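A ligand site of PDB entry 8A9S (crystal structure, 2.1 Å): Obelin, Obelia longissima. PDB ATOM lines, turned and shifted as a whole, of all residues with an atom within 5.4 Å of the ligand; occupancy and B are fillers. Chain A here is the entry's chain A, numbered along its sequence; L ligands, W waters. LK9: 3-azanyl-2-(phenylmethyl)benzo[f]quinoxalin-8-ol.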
ATOM      1  N   HIS A  22     -19.386  27.347  24.801  1.00  0.00           N
ATOM      2  CA  HIS A  22     -18.047  26.814  24.617  1.00  0.00           C
ATOM      3  C   HIS A  22     -17.882  25.417  25.219  1.00  0.00           C
ATOM      4  O   HIS A  22     -17.023  24.660  24.761  1.00  0.00           O
ATOM      5  CB  HIS A  22     -17.024  27.778  25.219  1.00  0.00           C
ATOM      6  CG  HIS A  22     -16.965  29.085  24.490  1.00  0.00           C
ATOM      7  ND1 HIS A  22     -16.372  29.213  23.261  1.00  0.00           N
ATOM      8  CD2 HIS A  22     -17.457  30.301  24.809  1.00  0.00           C
ATOM      9  CE1 HIS A  22     -16.482  30.463  22.851  1.00  0.00           C
ATOM     10  NE2 HIS A  22     -17.134  31.145  23.770  1.00  0.00           N
ATOM     11  N   MET A  25     -18.880  23.172  22.398  1.00  0.00           N
ATOM     12  CA  MET A  25     -17.804  23.010  21.417  1.00  0.00           C
ATOM     13  C   MET A  25     -16.620  22.243  21.997  1.00  0.00           C
ATOM     14  O   MET A  25     -15.967  21.487  21.279  1.00  0.00           O
ATOM     15  CB  MET A  25     -17.359  24.372  20.898  1.00  0.00           C
ATOM     16  CG  MET A  25     -18.471  25.180  20.220  1.00  0.00           C
ATOM     17  SD  MET A  25     -19.209  24.312  18.819  1.00  0.00           S
ATOM     18  CE  MET A  25     -17.808  24.170  17.713  1.00  0.00           C
ATOM     19  N   PHE A  26     -16.323  22.442  23.281  1.00  0.00           N
ATOM     20  CA  PHE A  26     -15.252  21.673  23.894  1.00  0.00           C
ATOM     21  C   PHE A  26     -15.535  20.173  23.805  1.00  0.00           C
ATOM     22  O   PHE A  26     -14.683  19.391  23.389  1.00  0.00           O
ATOM     23  CB  PHE A  26     -15.060  22.106  25.355  1.00  0.00           C
ATOM     24  CG  PHE A  26     -13.889  21.446  26.024  1.00  0.00           C
ATOM     25  CD1 PHE A  26     -14.029  20.226  26.674  1.00  0.00           C
ATOM     26  CD2 PHE A  26     -12.632  22.032  25.996  1.00  0.00           C
ATOM     27  CE1 PHE A  26     -12.950  19.609  27.281  1.00  0.00           C
ATOM     28  CE2 PHE A  26     -11.550  21.427  26.609  1.00  0.00           C
ATOM     29  CZ  PHE A  26     -11.711  20.209  27.249  1.00  0.00           C
ATOM     30  N   PHE A  28     -17.358  18.740  21.676  1.00  0.00           N
ATOM     31  CA  PHE A  28     -17.188  18.389  20.265  1.00  0.00           C
ATOM     32  C   PHE A  28     -15.714  18.134  19.950  1.00  0.00           C
ATOM     33  O   PHE A  28     -15.388  17.153  19.264  1.00  0.00           O
ATOM     34  CB  PHE A  28     -17.745  19.507  19.390  1.00  0.00           C
ATOM     35  CG  PHE A  28     -17.357  19.400  17.950  1.00  0.00           C
ATOM     36  CD1 PHE A  28     -17.958  18.467  17.122  1.00  0.00           C
ATOM     37  CD2 PHE A  28     -16.394  20.244  17.419  1.00  0.00           C
ATOM     38  CE1 PHE A  28     -17.597  18.376  15.785  1.00  0.00           C
ATOM     39  CE2 PHE A  28     -16.042  20.159  16.092  1.00  0.00           C
ATOM     40  CZ  PHE A  28     -16.635  19.219  15.277  1.00  0.00           C
ATOM     41  N   LEU A  29     -14.821  18.997  20.442  1.00  0.00           N
ATOM     42  CA  LEU A  29     -13.398  18.746  20.270  1.00  0.00           C
ATOM     43  C   LEU A  29     -12.938  17.535  21.072  1.00  0.00           C
ATOM     44  O   LEU A  29     -12.013  16.832  20.651  1.00  0.00           O
ATOM     45  CB  LEU A  29     -12.593  19.987  20.678  1.00  0.00           C
ATOM     46  CG  LEU A  29     -12.920  21.278  19.939  1.00  0.00           C
ATOM     47  CD1 LEU A  29     -12.058  22.418  20.434  1.00  0.00           C
ATOM     48  CD2 LEU A  29     -12.729  21.088  18.443  1.00  0.00           C
ATOM     49  N   ALA A  46      -9.450  20.153  13.236  1.00  0.00           N
ATOM     50  CA  ALA A  46     -10.090  21.390  12.840  1.00  0.00           C
ATOM     51  C   ALA A  46      -9.385  22.112  11.692  1.00  0.00           C
ATOM     52  O   ALA A  46      -9.895  23.135  11.237  1.00  0.00           O
ATOM     53  CB  ALA A  46     -10.209  22.338  14.034  1.00  0.00           C
ATOM     54  N   PHE A  72      -6.231  29.458  18.718  1.00  0.00           N
ATOM     55  CA  PHE A  72      -6.289  28.723  19.969  1.00  0.00           C
ATOM     56  C   PHE A  72      -5.039  28.888  20.826  1.00  0.00           C
ATOM     57  O   PHE A  72      -5.069  28.500  21.993  1.00  0.00           O
ATOM     58  CB  PHE A  72      -6.565  27.252  19.684  1.00  0.00           C
ATOM     59  CG  PHE A  72      -7.942  26.993  19.166  1.00  0.00           C
ATOM     60  CD1 PHE A  72      -9.025  27.005  20.023  1.00  0.00           C
ATOM     61  CD2 PHE A  72      -8.155  26.759  17.824  1.00  0.00           C
ATOM     62  CE1 PHE A  72     -10.300  26.785  19.555  1.00  0.00           C
ATOM     63  CE2 PHE A  72      -9.421  26.533  17.347  1.00  0.00           C
ATOM     64  CZ  PHE A  72     -10.501  26.558  18.209  1.00  0.00           C
ATOM     65  N   PHE A  88      -9.614  25.985  29.258  1.00  0.00           N
ATOM     66  CA  PHE A  88     -10.126  26.354  27.947  1.00  0.00           C
ATOM     67  C   PHE A  88     -11.014  27.596  28.026  1.00  0.00           C
ATOM     68  O   PHE A  88     -10.890  28.509  27.218  1.00  0.00           O
ATOM     69  CB  PHE A  88     -10.913  25.180  27.361  1.00  0.00           C
ATOM     70  CG  PHE A  88     -11.329  25.359  25.921  1.00  0.00           C
ATOM     71  CD1 PHE A  88     -10.421  25.189  24.896  1.00  0.00           C
ATOM     72  CD2 PHE A  88     -12.638  25.691  25.609  1.00  0.00           C
ATOM     73  CE1 PHE A  88     -10.803  25.344  23.580  1.00  0.00           C
ATOM     74  CE2 PHE A  88     -13.028  25.848  24.293  1.00  0.00           C
ATOM     75  CZ  PHE A  88     -12.103  25.664  23.272  1.00  0.00           C
ATOM     76  N   TRP A  92     -10.627  31.565  26.726  1.00  0.00           N
ATOM     77  CA  TRP A  92     -11.604  32.255  25.875  1.00  0.00           C
ATOM     78  C   TRP A  92     -11.931  33.636  26.426  1.00  0.00           C
ATOM     79  O   TRP A  92     -12.153  34.570  25.665  1.00  0.00           O
ATOM     80  CB  TRP A  92     -12.864  31.414  25.744  1.00  0.00           C
ATOM     81  CG  TRP A  92     -12.877  30.557  24.527  1.00  0.00           C
ATOM     82  CD1 TRP A  92     -12.522  29.250  24.440  1.00  0.00           C
ATOM     83  CD2 TRP A  92     -13.255  30.966  23.210  1.00  0.00           C
ATOM     84  NE1 TRP A  92     -12.665  28.808  23.150  1.00  0.00           N
ATOM     85  CE2 TRP A  92     -13.108  29.846  22.370  1.00  0.00           C
ATOM     86  CE3 TRP A  92     -13.708  32.168  22.658  1.00  0.00           C
ATOM     87  CZ2 TRP A  92     -13.406  29.885  21.016  1.00  0.00           C
ATOM     88  CZ3 TRP A  92     -14.005  32.208  21.304  1.00  0.00           C
ATOM     89  CH2 TRP A  92     -13.844  31.066  20.503  1.00  0.00           C
ATOM     90  N   ILE A 111     -10.059  36.049  15.015  1.00  0.00           N
ATOM     91  CA  ILE A 111     -11.304  35.503  14.477  1.00  0.00           C
ATOM     92  C   ILE A 111     -11.464  35.915  13.008  1.00  0.00           C
ATOM     93  O   ILE A 111     -11.887  35.109  12.167  1.00  0.00           O
ATOM     94  CB  ILE A 111     -12.513  35.946  15.329  1.00  0.00           C
ATOM     95  CG1 ILE A 111     -13.810  35.320  14.806  1.00  0.00           C
ATOM     96  CG2 ILE A 111     -12.664  37.445  15.333  1.00  0.00           C
ATOM     97  CD1 ILE A 111     -13.857  33.819  14.942  1.00  0.00           C
ATOM     98  N   TRP A 114      -8.941  33.910  10.791  1.00  0.00           N
ATOM     99  CA  TRP A 114      -9.521  32.585  10.641  1.00  0.00           C
ATOM    100  C   TRP A 114     -10.600  32.598   9.568  1.00  0.00           C
ATOM    101  O   TRP A 114     -10.593  31.776   8.637  1.00  0.00           O
ATOM    102  CB  TRP A 114     -10.091  32.104  11.973  1.00  0.00           C
ATOM    103  CG  TRP A 114     -10.485  30.660  12.002  1.00  0.00           C
ATOM    104  CD1 TRP A 114     -10.376  29.754  10.985  1.00  0.00           C
ATOM    105  CD2 TRP A 114     -11.051  29.952  13.108  1.00  0.00           C
ATOM    106  NE1 TRP A 114     -10.838  28.528  11.389  1.00  0.00           N
ATOM    107  CE2 TRP A 114     -11.260  28.619  12.688  1.00  0.00           C
ATOM    108  CE3 TRP A 114     -11.396  30.305  14.417  1.00  0.00           C
ATOM    109  CZ2 TRP A 114     -11.801  27.649  13.528  1.00  0.00           C
ATOM    110  CZ3 TRP A 114     -11.935  29.344  15.253  1.00  0.00           C
ATOM    111  CH2 TRP A 114     -12.129  28.028  14.803  1.00  0.00           C
ATOM    112  N   GLY A 115     -11.532  33.548   9.668  1.00  0.00           N
ATOM    113  CA  GLY A 115     -12.562  33.673   8.654  1.00  0.00           C
ATOM    114  C   GLY A 115     -11.999  33.883   7.257  1.00  0.00           C
ATOM    115  O   GLY A 115     -12.494  33.320   6.285  1.00  0.00           O
ATOM    116  N   VAL A 118     -10.855  30.582   5.777  1.00  0.00           N
ATOM    117  CA  VAL A 118     -11.965  29.721   5.369  1.00  0.00           C
ATOM    118  C   VAL A 118     -12.591  30.248   4.074  1.00  0.00           C
ATOM    119  O   VAL A 118     -12.783  29.498   3.112  1.00  0.00           O
ATOM    120  CB  VAL A 118     -13.004  29.624   6.501  1.00  0.00           C
ATOM    121  CG1 VAL A 118     -14.198  28.796   6.068  1.00  0.00           C
ATOM    122  CG2 VAL A 118     -12.371  29.003   7.736  1.00  0.00           C
ATOM    123  N   TRP A 135     -21.485  26.468   2.207  1.00  0.00           N
ATOM    124  CA  TRP A 135     -21.551  26.421   3.665  1.00  0.00           C
ATOM    125  C   TRP A 135     -22.019  25.050   4.147  1.00  0.00           C
ATOM    126  O   TRP A 135     -21.473  24.494   5.106  1.00  0.00           O
ATOM    127  CB  TRP A 135     -22.464  27.530   4.186  1.00  0.00           C
ATOM    128  CG  TRP A 135     -22.473  27.664   5.686  1.00  0.00           C
ATOM    129  CD1 TRP A 135     -23.462  27.281   6.535  1.00  0.00           C
ATOM    130  CD2 TRP A 135     -21.432  28.220   6.498  1.00  0.00           C
ATOM    131  NE1 TRP A 135     -23.113  27.562   7.835  1.00  0.00           N
ATOM    132  CE2 TRP A 135     -21.868  28.144   7.842  1.00  0.00           C
ATOM    133  CE3 TRP A 135     -20.183  28.778   6.234  1.00  0.00           C
ATOM    134  CZ2 TRP A 135     -21.102  28.597   8.905  1.00  0.00           C
ATOM    135  CZ3 TRP A 135     -19.418  29.228   7.287  1.00  0.00           C
ATOM    136  CH2 TRP A 135     -19.878  29.137   8.607  1.00  0.00           C
ATOM    137  N   TYR A 138     -19.090  22.917   4.105  1.00  0.00           N
ATOM    138  CA  TYR A 138     -18.207  23.262   5.220  1.00  0.00           C
ATOM    139  C   TYR A 138     -18.796  22.791   6.538  1.00  0.00           C
ATOM    140  O   TYR A 138     -18.128  22.104   7.311  1.00  0.00           O
ATOM    141  CB  TYR A 138     -17.963  24.767   5.246  1.00  0.00           C
ATOM    142  CG  TYR A 138     -17.090  25.199   6.404  1.00  0.00           C
ATOM    143  CD1 TYR A 138     -15.711  25.018   6.371  1.00  0.00           C
ATOM    144  CD2 TYR A 138     -17.644  25.778   7.537  1.00  0.00           C
ATOM    145  CE1 TYR A 138     -14.911  25.403   7.424  1.00  0.00           C
ATOM    146  CE2 TYR A 138     -16.856  26.161   8.604  1.00  0.00           C
ATOM    147  CZ  TYR A 138     -15.489  25.971   8.543  1.00  0.00           C
ATOM    148  OH  TYR A 138     -14.689  26.360   9.605  1.00  0.00           O
ATOM    149  N   SER A 142     -16.509  20.460   8.706  1.00  0.00           N
ATOM    150  CA  SER A 142     -15.981  20.996   9.954  1.00  0.00           C
ATOM    151  C   SER A 142     -16.769  20.512  11.168  1.00  0.00           C
ATOM    152  O   SER A 142     -16.258  20.576  12.288  1.00  0.00           O
ATOM    153  CB  SER A 142     -15.999  22.527   9.931  1.00  0.00           C
ATOM    154  OG  SER A 142     -17.329  23.014  10.035  1.00  0.00           O
ATOM    155  N   ILE A 144     -19.294  22.020  12.371  1.00  0.00           N
ATOM    156  CA  ILE A 144     -19.947  23.136  13.047  1.00  0.00           C
ATOM    157  C   ILE A 144     -21.437  23.124  12.757  1.00  0.00           C
ATOM    158  O   ILE A 144     -22.244  23.605  13.576  1.00  0.00           O
ATOM    159  CB  ILE A 144     -19.304  24.466  12.628  1.00  0.00           C
ATOM    160  CG1 ILE A 144     -19.780  25.625  13.517  1.00  0.00           C
ATOM    161  CG2 ILE A 144     -19.632  24.785  11.179  1.00  0.00           C
ATOM    162  CD1 ILE A 144     -19.223  25.594  14.918  1.00  0.00           C
ATOM    163  N   MET A 171     -20.114  37.304   8.537  1.00  0.00           N
ATOM    164  CA  MET A 171     -19.920  36.139   9.391  1.00  0.00           C
ATOM    165  C   MET A 171     -19.005  36.452  10.558  1.00  0.00           C
ATOM    166  O   MET A 171     -19.196  35.921  11.656  1.00  0.00           O
ATOM    167  CB  MET A 171     -19.369  34.987   8.567  1.00  0.00           C
ATOM    168  CG  MET A 171     -19.199  33.691   9.334  1.00  0.00           C
ATOM    169  SD  MET A 171     -20.716  33.182  10.166  1.00  0.00           S
ATOM    170  CE  MET A 171     -21.799  32.857   8.783  1.00  0.00           C
ATOM    171  N   HIS A 175     -19.833  36.191  14.490  1.00  0.00           N
ATOM    172  CA  HIS A 175     -18.985  35.440  15.410  1.00  0.00           C
ATOM    173  C   HIS A 175     -18.662  36.261  16.653  1.00  0.00           C
ATOM    174  O   HIS A 175     -18.618  35.719  17.765  1.00  0.00           O
ATOM    175  CB  HIS A 175     -17.716  34.989  14.684  1.00  0.00           C
ATOM    176  CG  HIS A 175     -17.943  33.824  13.770  1.00  0.00           C
ATOM    177  ND1 HIS A 175     -17.033  33.463  12.797  1.00  0.00           N
ATOM    178  CD2 HIS A 175     -18.965  32.946  13.673  1.00  0.00           C
ATOM    179  CE1 HIS A 175     -17.489  32.412  12.151  1.00  0.00           C
ATOM    180  NE2 HIS A 175     -18.661  32.078  12.655  1.00  0.00           N
ATOM    181  N   TRP A 179     -19.667  34.149  19.901  1.00  0.00           N
ATOM    182  CA  TRP A 179     -18.607  33.500  20.662  1.00  0.00           C
ATOM    183  C   TRP A 179     -17.954  34.397  21.704  1.00  0.00           C
ATOM    184  O   TRP A 179     -17.419  33.874  22.684  1.00  0.00           O
ATOM    185  CB  TRP A 179     -17.522  32.976  19.725  1.00  0.00           C
ATOM    186  CG  TRP A 179     -18.013  32.026  18.710  1.00  0.00           C
ATOM    187  CD1 TRP A 179     -18.010  32.191  17.363  1.00  0.00           C
ATOM    188  CD2 TRP A 179     -18.575  30.733  18.944  1.00  0.00           C
ATOM    189  NE1 TRP A 179     -18.530  31.089  16.744  1.00  0.00           N
ATOM    190  CE2 TRP A 179     -18.892  30.175  17.695  1.00  0.00           C
ATOM    191  CE3 TRP A 179     -18.851  29.992  20.100  1.00  0.00           C
ATOM    192  CZ2 TRP A 179     -19.466  28.911  17.564  1.00  0.00           C
ATOM    193  CZ3 TRP A 179     -19.411  28.738  19.974  1.00  0.00           C
ATOM    194  CH2 TRP A 179     -19.719  28.220  18.719  1.00  0.00           C
ATOM    195  N   TYR A 190     -26.292  29.411  14.369  1.00  0.00           N
ATOM    196  CA  TYR A 190     -26.185  28.061  13.838  1.00  0.00           C
ATOM    197  C   TYR A 190     -27.481  27.283  13.998  1.00  0.00           C
ATOM    198  O   TYR A 190     -27.458  26.054  14.108  1.00  0.00           O
ATOM    199  CB  TYR A 190     -25.034  27.325  14.527  1.00  0.00           C
ATOM    200  CG  TYR A 190     -23.716  28.028  14.361  1.00  0.00           C
ATOM    201  CD1 TYR A 190     -22.998  27.921  13.179  1.00  0.00           C
ATOM    202  CD2 TYR A 190     -23.195  28.813  15.373  1.00  0.00           C
ATOM    203  CE1 TYR A 190     -21.799  28.566  13.015  1.00  0.00           C
ATOM    204  CE2 TYR A 190     -21.994  29.462  15.218  1.00  0.00           C
ATOM    205  CZ  TYR A 190     -21.292  29.336  14.034  1.00  0.00           C
ATOM    206  OH  TYR A 190     -20.094  29.975  13.883  1.00  0.00           O
HETATM  207  N1  LK9 L   1     -14.831  25.679  14.161  1.00  0.00           N
HETATM  208  C2  LK9 L   1     -14.123  24.794  16.202  1.00  0.00           C
HETATM  209  C4  LK9 L   1     -14.638  25.934  18.256  1.00  0.00           C
HETATM  210  C5  LK9 L   1     -14.560  26.005  19.632  1.00  0.00           C
HETATM  211  C6  LK9 L   1     -15.153  27.072  20.278  1.00  0.00           C
HETATM  212  C7  LK9 L   1     -15.822  28.076  19.598  1.00  0.00           C
HETATM  213  C8  LK9 L   1     -15.900  28.005  18.222  1.00  0.00           C
HETATM  214  C9  LK9 L   1     -15.307  26.937  17.544  1.00  0.00           C
HETATM  215  C10 LK9 L   1     -15.362  26.836  16.166  1.00  0.00           C
HETATM  216  C11 LK9 L   1     -16.060  27.721  14.211  1.00  0.00           C
HETATM  217  C12 LK9 L   1     -16.811  28.846  13.503  1.00  0.00           C
HETATM  218  C14 LK9 L   1     -14.834  30.059  12.696  1.00  0.00           C
HETATM  219  C15 LK9 L   1     -13.999  30.685  11.584  1.00  0.00           C
HETATM  220  C16 LK9 L   1     -14.413  30.633  10.342  1.00  0.00           C
HETATM  221  C17 LK9 L   1     -15.736  29.946  10.006  1.00  0.00           C
HETATM  222  C18 LK9 L   1     -16.456  29.406  10.966  1.00  0.00           C
HETATM  223  N   LK9 L   1     -15.562  26.593  12.068  1.00  0.00           N
HETATM  224  C   LK9 L   1     -15.475  26.660  13.520  1.00  0.00           C
HETATM  225  O   LK9 L   1     -15.078  27.132  21.680  1.00  0.00           O
HETATM  226  C1  LK9 L   1     -14.775  25.783  15.494  1.00  0.00           C
HETATM  227  C13 LK9 L   1     -15.965  29.476  12.409  1.00  0.00           C
HETATM  228  C3  LK9 L   1     -14.044  24.869  17.588  1.00  0.00           C
HETATM  229  N2  LK9 L   1     -15.987  27.772  15.509  1.00  0.00           N
HETATM  230  O   HOH W   1     -14.049  22.742  13.308  1.00  0.00           O
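OH of Tyr 138 is in hydrogen-bond range of N of the ligand, 2.6 Å away.
O of the ligand is in hydrogen-bond range of ND1 of His 22.
NE1 of Trp 92 lies within hydrogen-bond range of O of the ligand, at 3.3 Å.
O of Tyr 138 sits at hydrogen-bond distance from OG of Ser 142, at 3.0 Å.
NE2 of His 22 sits at hydrogen-bond distance from O of Trp 179 (3.0 Å).
A ring nitrogen (NE2) of His 175 sits at hydrogen-bond distance from the side-chain hydroxyl (OH) of Tyr 190 (2.8 Å).
The side-chain sulfur of Met 171 sits at hydrogen-bond distance from a ring nitrogen (NE2) of His 175, at 3.4 Å.
The indole nitrogen (NE1) of Trp 179 is in hydrogen-bond range of the side-chain hydroxyl (OH) of Tyr 190 (3.4 Å).
The backbone NH (N) of Ile 144 lies close to the side-chain hydroxyl (OG) of Ser 142 (3.2 Å).
Residues that only touch the ligand: Met 25 (3.5 Å), Phe 72 (3.97 Å), Phe 88 (3.6 Å), Trp 114 (3.4 Å), Gly 115 (3.9 Å), Val 118 (3.7 Å), Ile 144 (3.9 Å), His 175 (3.3 Å), Trp 179 (3.6 Å) and Tyr 190 (3.5 Å).
Hydrophobic or aromatic side chains that line the ligand: His 22, Met 25, Phe 72, Phe 88, Trp 92, Trp 114, Val 118, Tyr 138, Ile 144, His 175 and Trp 179.
13 residues have an atom within 4 Å of the ligand: His 22, Met 25, Phe 72, Phe 88, Trp 92, Trp 114, Gly 115, Val 118, Tyr 138, Ile 144, His 175, Trp 179 and Tyr 190.
Water W1 bridges a nitrogen (N1) of the ligand (3.2 Å) and the backbone carbonyl oxygen (O) of Ser 142 (3.3 Å).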
